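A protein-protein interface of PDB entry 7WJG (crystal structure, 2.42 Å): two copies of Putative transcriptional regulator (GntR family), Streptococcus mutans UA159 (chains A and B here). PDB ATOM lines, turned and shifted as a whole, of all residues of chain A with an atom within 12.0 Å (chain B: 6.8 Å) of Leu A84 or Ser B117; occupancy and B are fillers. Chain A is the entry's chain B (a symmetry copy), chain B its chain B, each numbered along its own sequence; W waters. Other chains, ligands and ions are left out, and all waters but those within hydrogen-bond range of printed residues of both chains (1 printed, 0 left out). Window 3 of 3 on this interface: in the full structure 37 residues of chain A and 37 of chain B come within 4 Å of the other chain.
The side-chain hydroxyl of Ser B114 lies within hydrogen-bond range of the side-chain amino group of Lys A88. The side-chain carboxylate of Asp B187 lies within hydrogen-bond range of the backbone NH of Leu A84 (2.6 Å). OG of Ser B191 sits at hydrogen-bond distance from N of Gly A83, 3.0 Å away.
No position is printed for both chains.
Printed residues of chain B that touch a printed residue of chain A: Leu B113, Ser B114, Ser B117, Asp B187, Phe B188 and Ser B191. Hydrophobic or aromatic side chains of chain A within 4 Å of the printed part of chain B: Ala A82, Leu A84 and Ile A91.
Water W1 lies within hydrogen-bond range of OD2 of Asp B187 (2.8 Å) and N of Lys A85 (3.3 Å).
Of chain B, only Ser B117 and Asp B187 come within 4 Å of Leu A84. Of chain A, only Leu A84 comes within 4 Å of Ser B117. Leu B113 touches just these residues of chain A: Lys A88 and Ile A91. Ser B114 touches just one residue of chain A: Lys A88. Ala B116 touches none of the printed residues of chain A. Ile B119 touches none of the printed residues of chain A. Printed residues of chain B within 4 Å of Ala A82: Phe B188 and Ser B191. Printed residues of chain B within 4 Å of Ile A91: Leu B113 (3.9 Å).
The backbone carbonyl oxygen (O) of Leu B113 lies within hydrogen-bond range of the side-chain hydroxyl (OG) of Ser B117 (2.7 Å). The backbone carbonyl oxygen (O) of Asp B187 is in hydrogen-bond range of the side-chain hydroxyl (OG) of Ser B191, at 3.4 Å. N of Ala A82 lies within hydrogen-bond range of OE2 of Glu A86 (3.4 Å).
O of Ala A82 touches CE1 of Phe B188, at 3.4 Å. Ala A82 touches Ser B191 (CA to CB, 3.6 Å). Gly A83 touches Asp B187 (CA to OD2, 3.3 Å). CD1 of Leu A84 touches CA of Ser B117, at 3.7 Å. CG of Lys A88 touches CD1 of Leu B113, 3.95 Å away. CD1 of Leu B113 touches CD1 of Ile A91 (3.9 Å).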
ATOM      1  N   ALA A  80      40.003  19.705   4.495  1.00  0.00           N
ATOM      2  CA  ALA A  80      39.459  19.831   3.155  1.00  0.00           C
ATOM      3  C   ALA A  80      38.325  20.848   3.136  1.00  0.00           C
ATOM      4  O   ALA A  80      37.630  21.058   4.133  1.00  0.00           O
ATOM      5  CB  ALA A  80      38.966  18.472   2.661  1.00  0.00           C
ATOM      6  N   THR A  81      38.144  21.490   1.988  1.00  0.00           N
ATOM      7  CA  THR A  81      37.101  22.501   1.860  1.00  0.00           C
ATOM      8  C   THR A  81      35.726  21.856   2.000  1.00  0.00           C
ATOM      9  O   THR A  81      35.455  20.790   1.434  1.00  0.00           O
ATOM     10  CB  THR A  81      37.231  23.236   0.517  1.00  0.00           C
ATOM     11  OG1 THR A  81      38.390  24.083   0.557  1.00  0.00           O
ATOM     12  CG2 THR A  81      35.990  24.097   0.222  1.00  0.00           C
ATOM     13  N   ALA A  82      34.861  22.507   2.774  1.00  0.00           N
ATOM     14  CA  ALA A  82      33.599  21.909   3.168  1.00  0.00           C
ATOM     15  C   ALA A  82      32.643  22.996   3.625  1.00  0.00           C
ATOM     16  O   ALA A  82      33.058  24.007   4.201  1.00  0.00           O
ATOM     17  CB  ALA A  82      33.807  20.873   4.287  1.00  0.00           C
ATOM     18  N   GLY A  83      31.359  22.761   3.386  1.00  0.00           N
ATOM     19  CA  GLY A  83      30.305  23.627   3.880  1.00  0.00           C
ATOM     20  C   GLY A  83      29.954  24.752   2.917  1.00  0.00           C
ATOM     21  O   GLY A  83      30.745  25.170   2.068  1.00  0.00           O
ATOM     22  N   LEU A  84      28.730  25.258   3.069  1.00  0.00           N
ATOM     23  CA  LEU A  84      28.223  26.251   2.129  1.00  0.00           C
ATOM     24  C   LEU A  84      29.018  27.552   2.212  1.00  0.00           C
ATOM     25  O   LEU A  84      29.279  28.192   1.185  1.00  0.00           O
ATOM     26  CB  LEU A  84      26.734  26.495   2.388  1.00  0.00           C
ATOM     27  CG  LEU A  84      25.809  25.363   1.922  1.00  0.00           C
ATOM     28  CD1 LEU A  84      24.333  25.669   2.207  1.00  0.00           C
ATOM     29  CD2 LEU A  84      26.038  25.039   0.440  1.00  0.00           C
ATOM     30  N   LYS A  85      29.431  27.943   3.425  1.00  0.00           N
ATOM     31  CA  LYS A  85      30.133  29.209   3.596  1.00  0.00           C
ATOM     32  C   LYS A  85      31.420  29.238   2.778  1.00  0.00           C
ATOM     33  O   LYS A  85      31.758  30.263   2.169  1.00  0.00           O
ATOM     34  CB  LYS A  85      30.410  29.455   5.080  1.00  0.00           C
ATOM     35  CG  LYS A  85      30.803  30.882   5.414  1.00  0.00           C
ATOM     36  CD  LYS A  85      31.352  30.996   6.843  1.00  0.00           C
ATOM     37  CE  LYS A  85      30.569  32.016   7.688  1.00  0.00           C
ATOM     38  NZ  LYS A  85      31.415  32.645   8.749  1.00  0.00           N
ATOM     39  N   GLU A  86      32.135  28.112   2.720  1.00  0.00           N
ATOM     40  CA  GLU A  86      33.357  28.067   1.919  1.00  0.00           C
ATOM     41  C   GLU A  86      33.041  28.116   0.432  1.00  0.00           C
ATOM     42  O   GLU A  86      33.751  28.776  -0.332  1.00  0.00           O
ATOM     43  CB  GLU A  86      34.176  26.818   2.251  1.00  0.00           C
ATOM     44  CG  GLU A  86      34.921  26.903   3.577  1.00  0.00           C
ATOM     45  CD  GLU A  86      36.042  25.885   3.687  1.00  0.00           C
ATOM     46  OE1 GLU A  86      36.917  25.875   2.790  1.00  0.00           O
ATOM     47  OE2 GLU A  86      36.044  25.097   4.667  1.00  0.00           O
ATOM     48  N   MET A  87      31.980  27.428   0.001  1.00  0.00           N
ATOM     49  CA  MET A  87      31.614  27.454  -1.412  1.00  0.00           C
ATOM     50  C   MET A  87      31.171  28.848  -1.843  1.00  0.00           C
ATOM     51  O   MET A  87      31.383  29.248  -2.997  1.00  0.00           O
ATOM     52  CB  MET A  87      30.516  26.428  -1.676  1.00  0.00           C
ATOM     53  CG  MET A  87      30.346  26.029  -3.145  1.00  0.00           C
ATOM     54  SD  MET A  87      29.424  24.468  -3.289  1.00  0.00           S
ATOM     55  CE  MET A  87      29.887  23.635  -1.753  1.00  0.00           C
ATOM     56  N   LYS A  88      30.568  29.598  -0.924  1.00  0.00           N
ATOM     57  CA  LYS A  88      30.216  30.982  -1.199  1.00  0.00           C
ATOM     58  C   LYS A  88      31.468  31.837  -1.352  1.00  0.00           C
ATOM     59  O   LYS A  88      31.583  32.617  -2.304  1.00  0.00           O
ATOM     60  CB  LYS A  88      29.308  31.502  -0.086  1.00  0.00           C
ATOM     61  CG  LYS A  88      29.031  32.983  -0.088  1.00  0.00           C
ATOM     62  CD  LYS A  88      28.137  33.337   1.103  1.00  0.00           C
ATOM     63  CE  LYS A  88      27.829  34.816   1.148  1.00  0.00           C
ATOM     64  NZ  LYS A  88      27.148  35.202   2.407  1.00  0.00           N
ATOM     65  N   GLN A  89      32.431  31.688  -0.441  1.00  0.00           N
ATOM     66  CA  GLN A  89      33.698  32.401  -0.600  1.00  0.00           C
ATOM     67  C   GLN A  89      34.395  32.007  -1.898  1.00  0.00           C
ATOM     68  O   GLN A  89      35.027  32.842  -2.555  1.00  0.00           O
ATOM     69  CB  GLN A  89      34.610  32.136   0.593  1.00  0.00           C
ATOM     70  CG  GLN A  89      34.155  32.799   1.886  1.00  0.00           C
ATOM     71  CD  GLN A  89      34.659  32.057   3.123  1.00  0.00           C
ATOM     72  OE1 GLN A  89      35.348  31.031   3.014  1.00  0.00           O
ATOM     73  NE2 GLN A  89      34.324  32.578   4.306  1.00  0.00           N
ATOM     74  N   ASP A  90      34.283  30.739  -2.279  1.00  0.00           N
ATOM     75  CA  ASP A  90      34.751  30.297  -3.584  1.00  0.00           C
ATOM     76  C   ASP A  90      34.115  31.110  -4.706  1.00  0.00           C
ATOM     77  O   ASP A  90      34.817  31.653  -5.565  1.00  0.00           O
ATOM     78  CB  ASP A  90      34.436  28.811  -3.752  1.00  0.00           C
ATOM     79  CG  ASP A  90      35.558  27.910  -3.277  1.00  0.00           C
ATOM     80  OD1 ASP A  90      36.340  28.318  -2.380  1.00  0.00           O
ATOM     81  OD2 ASP A  90      35.643  26.783  -3.812  1.00  0.00           O
ATOM     82  N   ILE A  91      32.781  31.198  -4.720  1.00  0.00           N
ATOM     83  CA  ILE A  91      32.106  31.955  -5.774  1.00  0.00           C
ATOM     84  C   ILE A  91      32.486  33.430  -5.698  1.00  0.00           C
ATOM     85  O   ILE A  91      32.700  34.086  -6.724  1.00  0.00           O
ATOM     86  CB  ILE A  91      30.582  31.751  -5.686  1.00  0.00           C
ATOM     87  CG1 ILE A  91      30.205  30.337  -6.138  1.00  0.00           C
ATOM     88  CG2 ILE A  91      29.838  32.807  -6.500  1.00  0.00           C
ATOM     89  CD1 ILE A  91      28.805  29.916  -5.716  1.00  0.00           C
ATOM     90  N   GLN A  92      32.606  33.969  -4.487  1.00  0.00           N
ATOM     91  CA  GLN A  92      32.970  35.373  -4.355  1.00  0.00           C
ATOM     92  C   GLN A  92      34.375  35.647  -4.886  1.00  0.00           C
ATOM     93  O   GLN A  92      34.612  36.690  -5.507  1.00  0.00           O
ATOM     94  CB  GLN A  92      32.840  35.809  -2.903  1.00  0.00           C
ATOM     95  CG  GLN A  92      31.398  36.066  -2.531  1.00  0.00           C
ATOM     96  CD  GLN A  92      31.185  36.186  -1.044  1.00  0.00           C
ATOM     97  OE1 GLN A  92      32.049  35.810  -0.248  1.00  0.00           O
ATOM     98  NE2 GLN A  92      30.025  36.710  -0.655  1.00  0.00           N
ATOM     99  N   ARG A  93      35.318  34.724  -4.664  1.00  0.00           N
ATOM    100  CA  ARG A  93      36.650  34.893  -5.242  1.00  0.00           C
ATOM    101  C   ARG A  93      36.583  34.944  -6.764  1.00  0.00           C
ATOM    102  O   ARG A  93      37.301  35.725  -7.401  1.00  0.00           O
ATOM    103  CB  ARG A  93      37.583  33.772  -4.782  1.00  0.00           C
ATOM    104  CG  ARG A  93      38.472  34.174  -3.592  1.00  0.00           C
ATOM    105  CD  ARG A  93      39.494  33.087  -3.253  1.00  0.00           C
ATOM    106  NE  ARG A  93      38.830  31.838  -2.894  1.00  0.00           N
ATOM    107  CZ  ARG A  93      38.344  31.573  -1.684  1.00  0.00           C
ATOM    108  NH1 ARG A  93      38.471  32.465  -0.705  1.00  0.00           N
ATOM    109  NH2 ARG A  93      37.734  30.413  -1.455  1.00  0.00           N
ATOM    110  N   PHE B 112      21.570  35.880  -2.855  1.00  0.00           N
ATOM    111  CA  PHE B 112      21.080  34.570  -3.254  1.00  0.00           C
ATOM    112  C   PHE B 112      21.736  33.462  -2.435  1.00  0.00           C
ATOM    113  O   PHE B 112      21.049  32.607  -1.859  1.00  0.00           O
ATOM    114  CB  PHE B 112      21.342  34.373  -4.739  1.00  0.00           C
ATOM    115  CG  PHE B 112      20.898  33.044  -5.272  1.00  0.00           C
ATOM    116  CD1 PHE B 112      19.544  32.777  -5.479  1.00  0.00           C
ATOM    117  CD2 PHE B 112      21.832  32.085  -5.630  1.00  0.00           C
ATOM    118  CE1 PHE B 112      19.140  31.555  -6.011  1.00  0.00           C
ATOM    119  CE2 PHE B 112      21.437  30.861  -6.161  1.00  0.00           C
ATOM    120  CZ  PHE B 112      20.090  30.592  -6.346  1.00  0.00           C
ATOM    121  N   LEU B 113      23.072  33.463  -2.371  1.00  0.00           N
ATOM    122  CA  LEU B 113      23.795  32.392  -1.685  1.00  0.00           C
ATOM    123  C   LEU B 113      23.562  32.425  -0.181  1.00  0.00           C
ATOM    124  O   LEU B 113      23.545  31.369   0.458  1.00  0.00           O
ATOM    125  CB  LEU B 113      25.295  32.492  -1.982  1.00  0.00           C
ATOM    126  CG  LEU B 113      25.729  32.361  -3.440  1.00  0.00           C
ATOM    127  CD1 LEU B 113      27.206  32.698  -3.583  1.00  0.00           C
ATOM    128  CD2 LEU B 113      25.428  30.968  -4.021  1.00  0.00           C
ATOM    129  N   SER B 114      23.398  33.619   0.397  1.00  0.00           N
ATOM    130  CA  SER B 114      23.167  33.742   1.828  1.00  0.00           C
ATOM    131  C   SER B 114      21.816  33.172   2.224  1.00  0.00           C
ATOM    132  O   SER B 114      21.691  32.531   3.270  1.00  0.00           O
ATOM    133  CB  SER B 114      23.268  35.205   2.236  1.00  0.00           C
ATOM    134  OG  SER B 114      24.603  35.644   2.068  1.00  0.00           O
ATOM    135  N   GLN B 115      20.794  33.396   1.404  1.00  0.00           N
ATOM    136  CA  GLN B 115      19.473  32.908   1.759  1.00  0.00           C
ATOM    137  C   GLN B 115      19.339  31.421   1.430  1.00  0.00           C
ATOM    138  O   GLN B 115      18.717  30.664   2.185  1.00  0.00           O
ATOM    139  CB  GLN B 115      18.401  33.751   1.052  1.00  0.00           C
ATOM    140  CG  GLN B 115      16.958  33.287   1.273  1.00  0.00           C
ATOM    141  CD  GLN B 115      15.964  33.979   0.335  1.00  0.00           C
ATOM    142  OE1 GLN B 115      14.953  33.386  -0.073  1.00  0.00           O
ATOM    143  NE2 GLN B 115      16.248  35.240  -0.006  1.00  0.00           N
ATOM    144  N   ALA B 116      19.946  30.966   0.337  1.00  0.00           N
ATOM    145  CA  ALA B 116      19.878  29.538   0.052  1.00  0.00           C
ATOM    146  C   ALA B 116      20.607  28.735   1.126  1.00  0.00           C
ATOM    147  O   ALA B 116      20.272  27.570   1.378  1.00  0.00           O
ATOM    148  CB  ALA B 116      20.459  29.241  -1.338  1.00  0.00           C
ATOM    149  N   SER B 117      21.598  29.354   1.769  1.00  0.00           N
ATOM    150  CA  SER B 117      22.306  28.710   2.861  1.00  0.00           C
ATOM    151  C   SER B 117      21.370  28.390   4.007  1.00  0.00           C
ATOM    152  O   SER B 117      21.563  27.396   4.714  1.00  0.00           O
ATOM    153  CB  SER B 117      23.438  29.612   3.331  1.00  0.00           C
ATOM    154  OG  SER B 117      24.425  29.684   2.327  1.00  0.00           O
ATOM    155  N   LEU B 118      20.331  29.197   4.172  1.00  0.00           N
ATOM    156  CA  LEU B 118      19.377  29.036   5.248  1.00  0.00           C
ATOM    157  C   LEU B 118      18.302  28.002   4.963  1.00  0.00           C
ATOM    158  O   LEU B 118      17.538  27.686   5.875  1.00  0.00           O
ATOM    159  CB  LEU B 118      18.693  30.371   5.532  1.00  0.00           C
ATOM    160  CG  LEU B 118      19.539  31.570   5.935  1.00  0.00           C
ATOM    161  CD1 LEU B 118      18.614  32.769   6.112  1.00  0.00           C
ATOM    162  CD2 LEU B 118      20.307  31.268   7.204  1.00  0.00           C
ATOM    163  N   ILE B 119      18.191  27.489   3.735  1.00  0.00           N
ATOM    164  CA  ILE B 119      17.024  26.673   3.397  1.00  0.00           C
ATOM    165  C   ILE B 119      16.850  25.550   4.405  1.00  0.00           C
ATOM    166  O   ILE B 119      15.769  25.367   4.977  1.00  0.00           O
ATOM    167  CB  ILE B 119      17.128  26.113   1.972  1.00  0.00           C
ATOM    168  CG1 ILE B 119      16.835  27.195   0.929  1.00  0.00           C
ATOM    169  CG2 ILE B 119      16.158  24.937   1.806  1.00  0.00           C
ATOM    170  CD1 ILE B 119      17.231  26.761  -0.483  1.00  0.00           C
ATOM    171  N   ARG B 120      17.923  24.807   4.670  1.00  0.00           N
ATOM    172  CA  ARG B 120      17.809  23.598   5.477  1.00  0.00           C
ATOM    173  C   ARG B 120      17.805  23.851   6.977  1.00  0.00           C
ATOM    174  O   ARG B 120      17.679  22.882   7.728  1.00  0.00           O
ATOM    175  CB  ARG B 120      18.937  22.627   5.131  1.00  0.00           C
ATOM    176  CG  ARG B 120      18.629  21.797   3.911  1.00  0.00           C
ATOM    177  CD  ARG B 120      19.821  20.964   3.563  1.00  0.00           C
ATOM    178  NE  ARG B 120      19.518  19.974   2.538  1.00  0.00           N
ATOM    179  CZ  ARG B 120      19.095  18.744   2.800  1.00  0.00           C
ATOM    180  NH1 ARG B 120      18.925  18.362   4.058  1.00  0.00           N
ATOM    181  NH2 ARG B 120      18.847  17.901   1.808  1.00  0.00           N
ATOM    182  N   LYS B 121      17.912  25.108   7.430  1.00  0.00           N
ATOM    183  CA  LYS B 121      18.120  25.374   8.854  1.00  0.00           C
ATOM    184  C   LYS B 121      16.957  24.873   9.705  1.00  0.00           C
ATOM    185  O   LYS B 121      17.167  24.340  10.804  1.00  0.00           O
ATOM    186  CB  LYS B 121      18.343  26.864   9.106  1.00  0.00           C
ATOM    187  CG  LYS B 121      18.553  27.174  10.589  1.00  0.00           C
ATOM    188  CD  LYS B 121      19.068  28.593  10.836  1.00  0.00           C
ATOM    189  CE  LYS B 121      17.962  29.531  11.346  1.00  0.00           C
ATOM    190  NZ  LYS B 121      18.442  30.938  11.521  1.00  0.00           N
ATOM    191  N   ASP B 187      25.718  21.186   6.686  1.00  0.00           N
ATOM    192  CA  ASP B 187      26.267  21.294   5.331  1.00  0.00           C
ATOM    193  C   ASP B 187      27.716  20.820   5.276  1.00  0.00           C
ATOM    194  O   ASP B 187      28.149  20.298   4.247  1.00  0.00           O
ATOM    195  CB  ASP B 187      26.146  22.732   4.810  1.00  0.00           C
ATOM    196  CG  ASP B 187      26.786  23.752   5.755  1.00  0.00           C
ATOM    197  OD1 ASP B 187      26.590  23.617   6.973  1.00  0.00           O
ATOM    198  OD2 ASP B 187      27.485  24.680   5.290  1.00  0.00           O
ATOM    199  N   PHE B 188      28.473  20.982   6.366  1.00  0.00           N
ATOM    200  CA  PHE B 188      29.799  20.376   6.435  1.00  0.00           C
ATOM    201  C   PHE B 188      29.717  18.867   6.305  1.00  0.00           C
ATOM    202  O   PHE B 188      30.539  18.248   5.620  1.00  0.00           O
ATOM    203  CB  PHE B 188      30.489  20.734   7.743  1.00  0.00           C
ATOM    204  CG  PHE B 188      30.811  22.175   7.874  1.00  0.00           C
ATOM    205  CD1 PHE B 188      32.014  22.674   7.409  1.00  0.00           C
ATOM    206  CD2 PHE B 188      29.914  23.035   8.465  1.00  0.00           C
ATOM    207  CE1 PHE B 188      32.317  24.010   7.539  1.00  0.00           C
ATOM    208  CE2 PHE B 188      30.203  24.370   8.594  1.00  0.00           C
ATOM    209  CZ  PHE B 188      31.409  24.856   8.141  1.00  0.00           C
ATOM    210  N   SER B 191      29.453  17.865   2.575  1.00  0.00           N
ATOM    211  CA  SER B 191      30.726  17.954   1.857  1.00  0.00           C
ATOM    212  C   SER B 191      31.679  16.848   2.277  1.00  0.00           C
ATOM    213  O   SER B 191      32.419  16.302   1.454  1.00  0.00           O
ATOM    214  CB  SER B 191      31.393  19.311   2.112  1.00  0.00           C
ATOM    215  OG  SER B 191      30.537  20.391   1.806  1.00  0.00           O
HETATM  216  O   HOH W   1      29.419  26.470   6.333  1.00  0.00           O
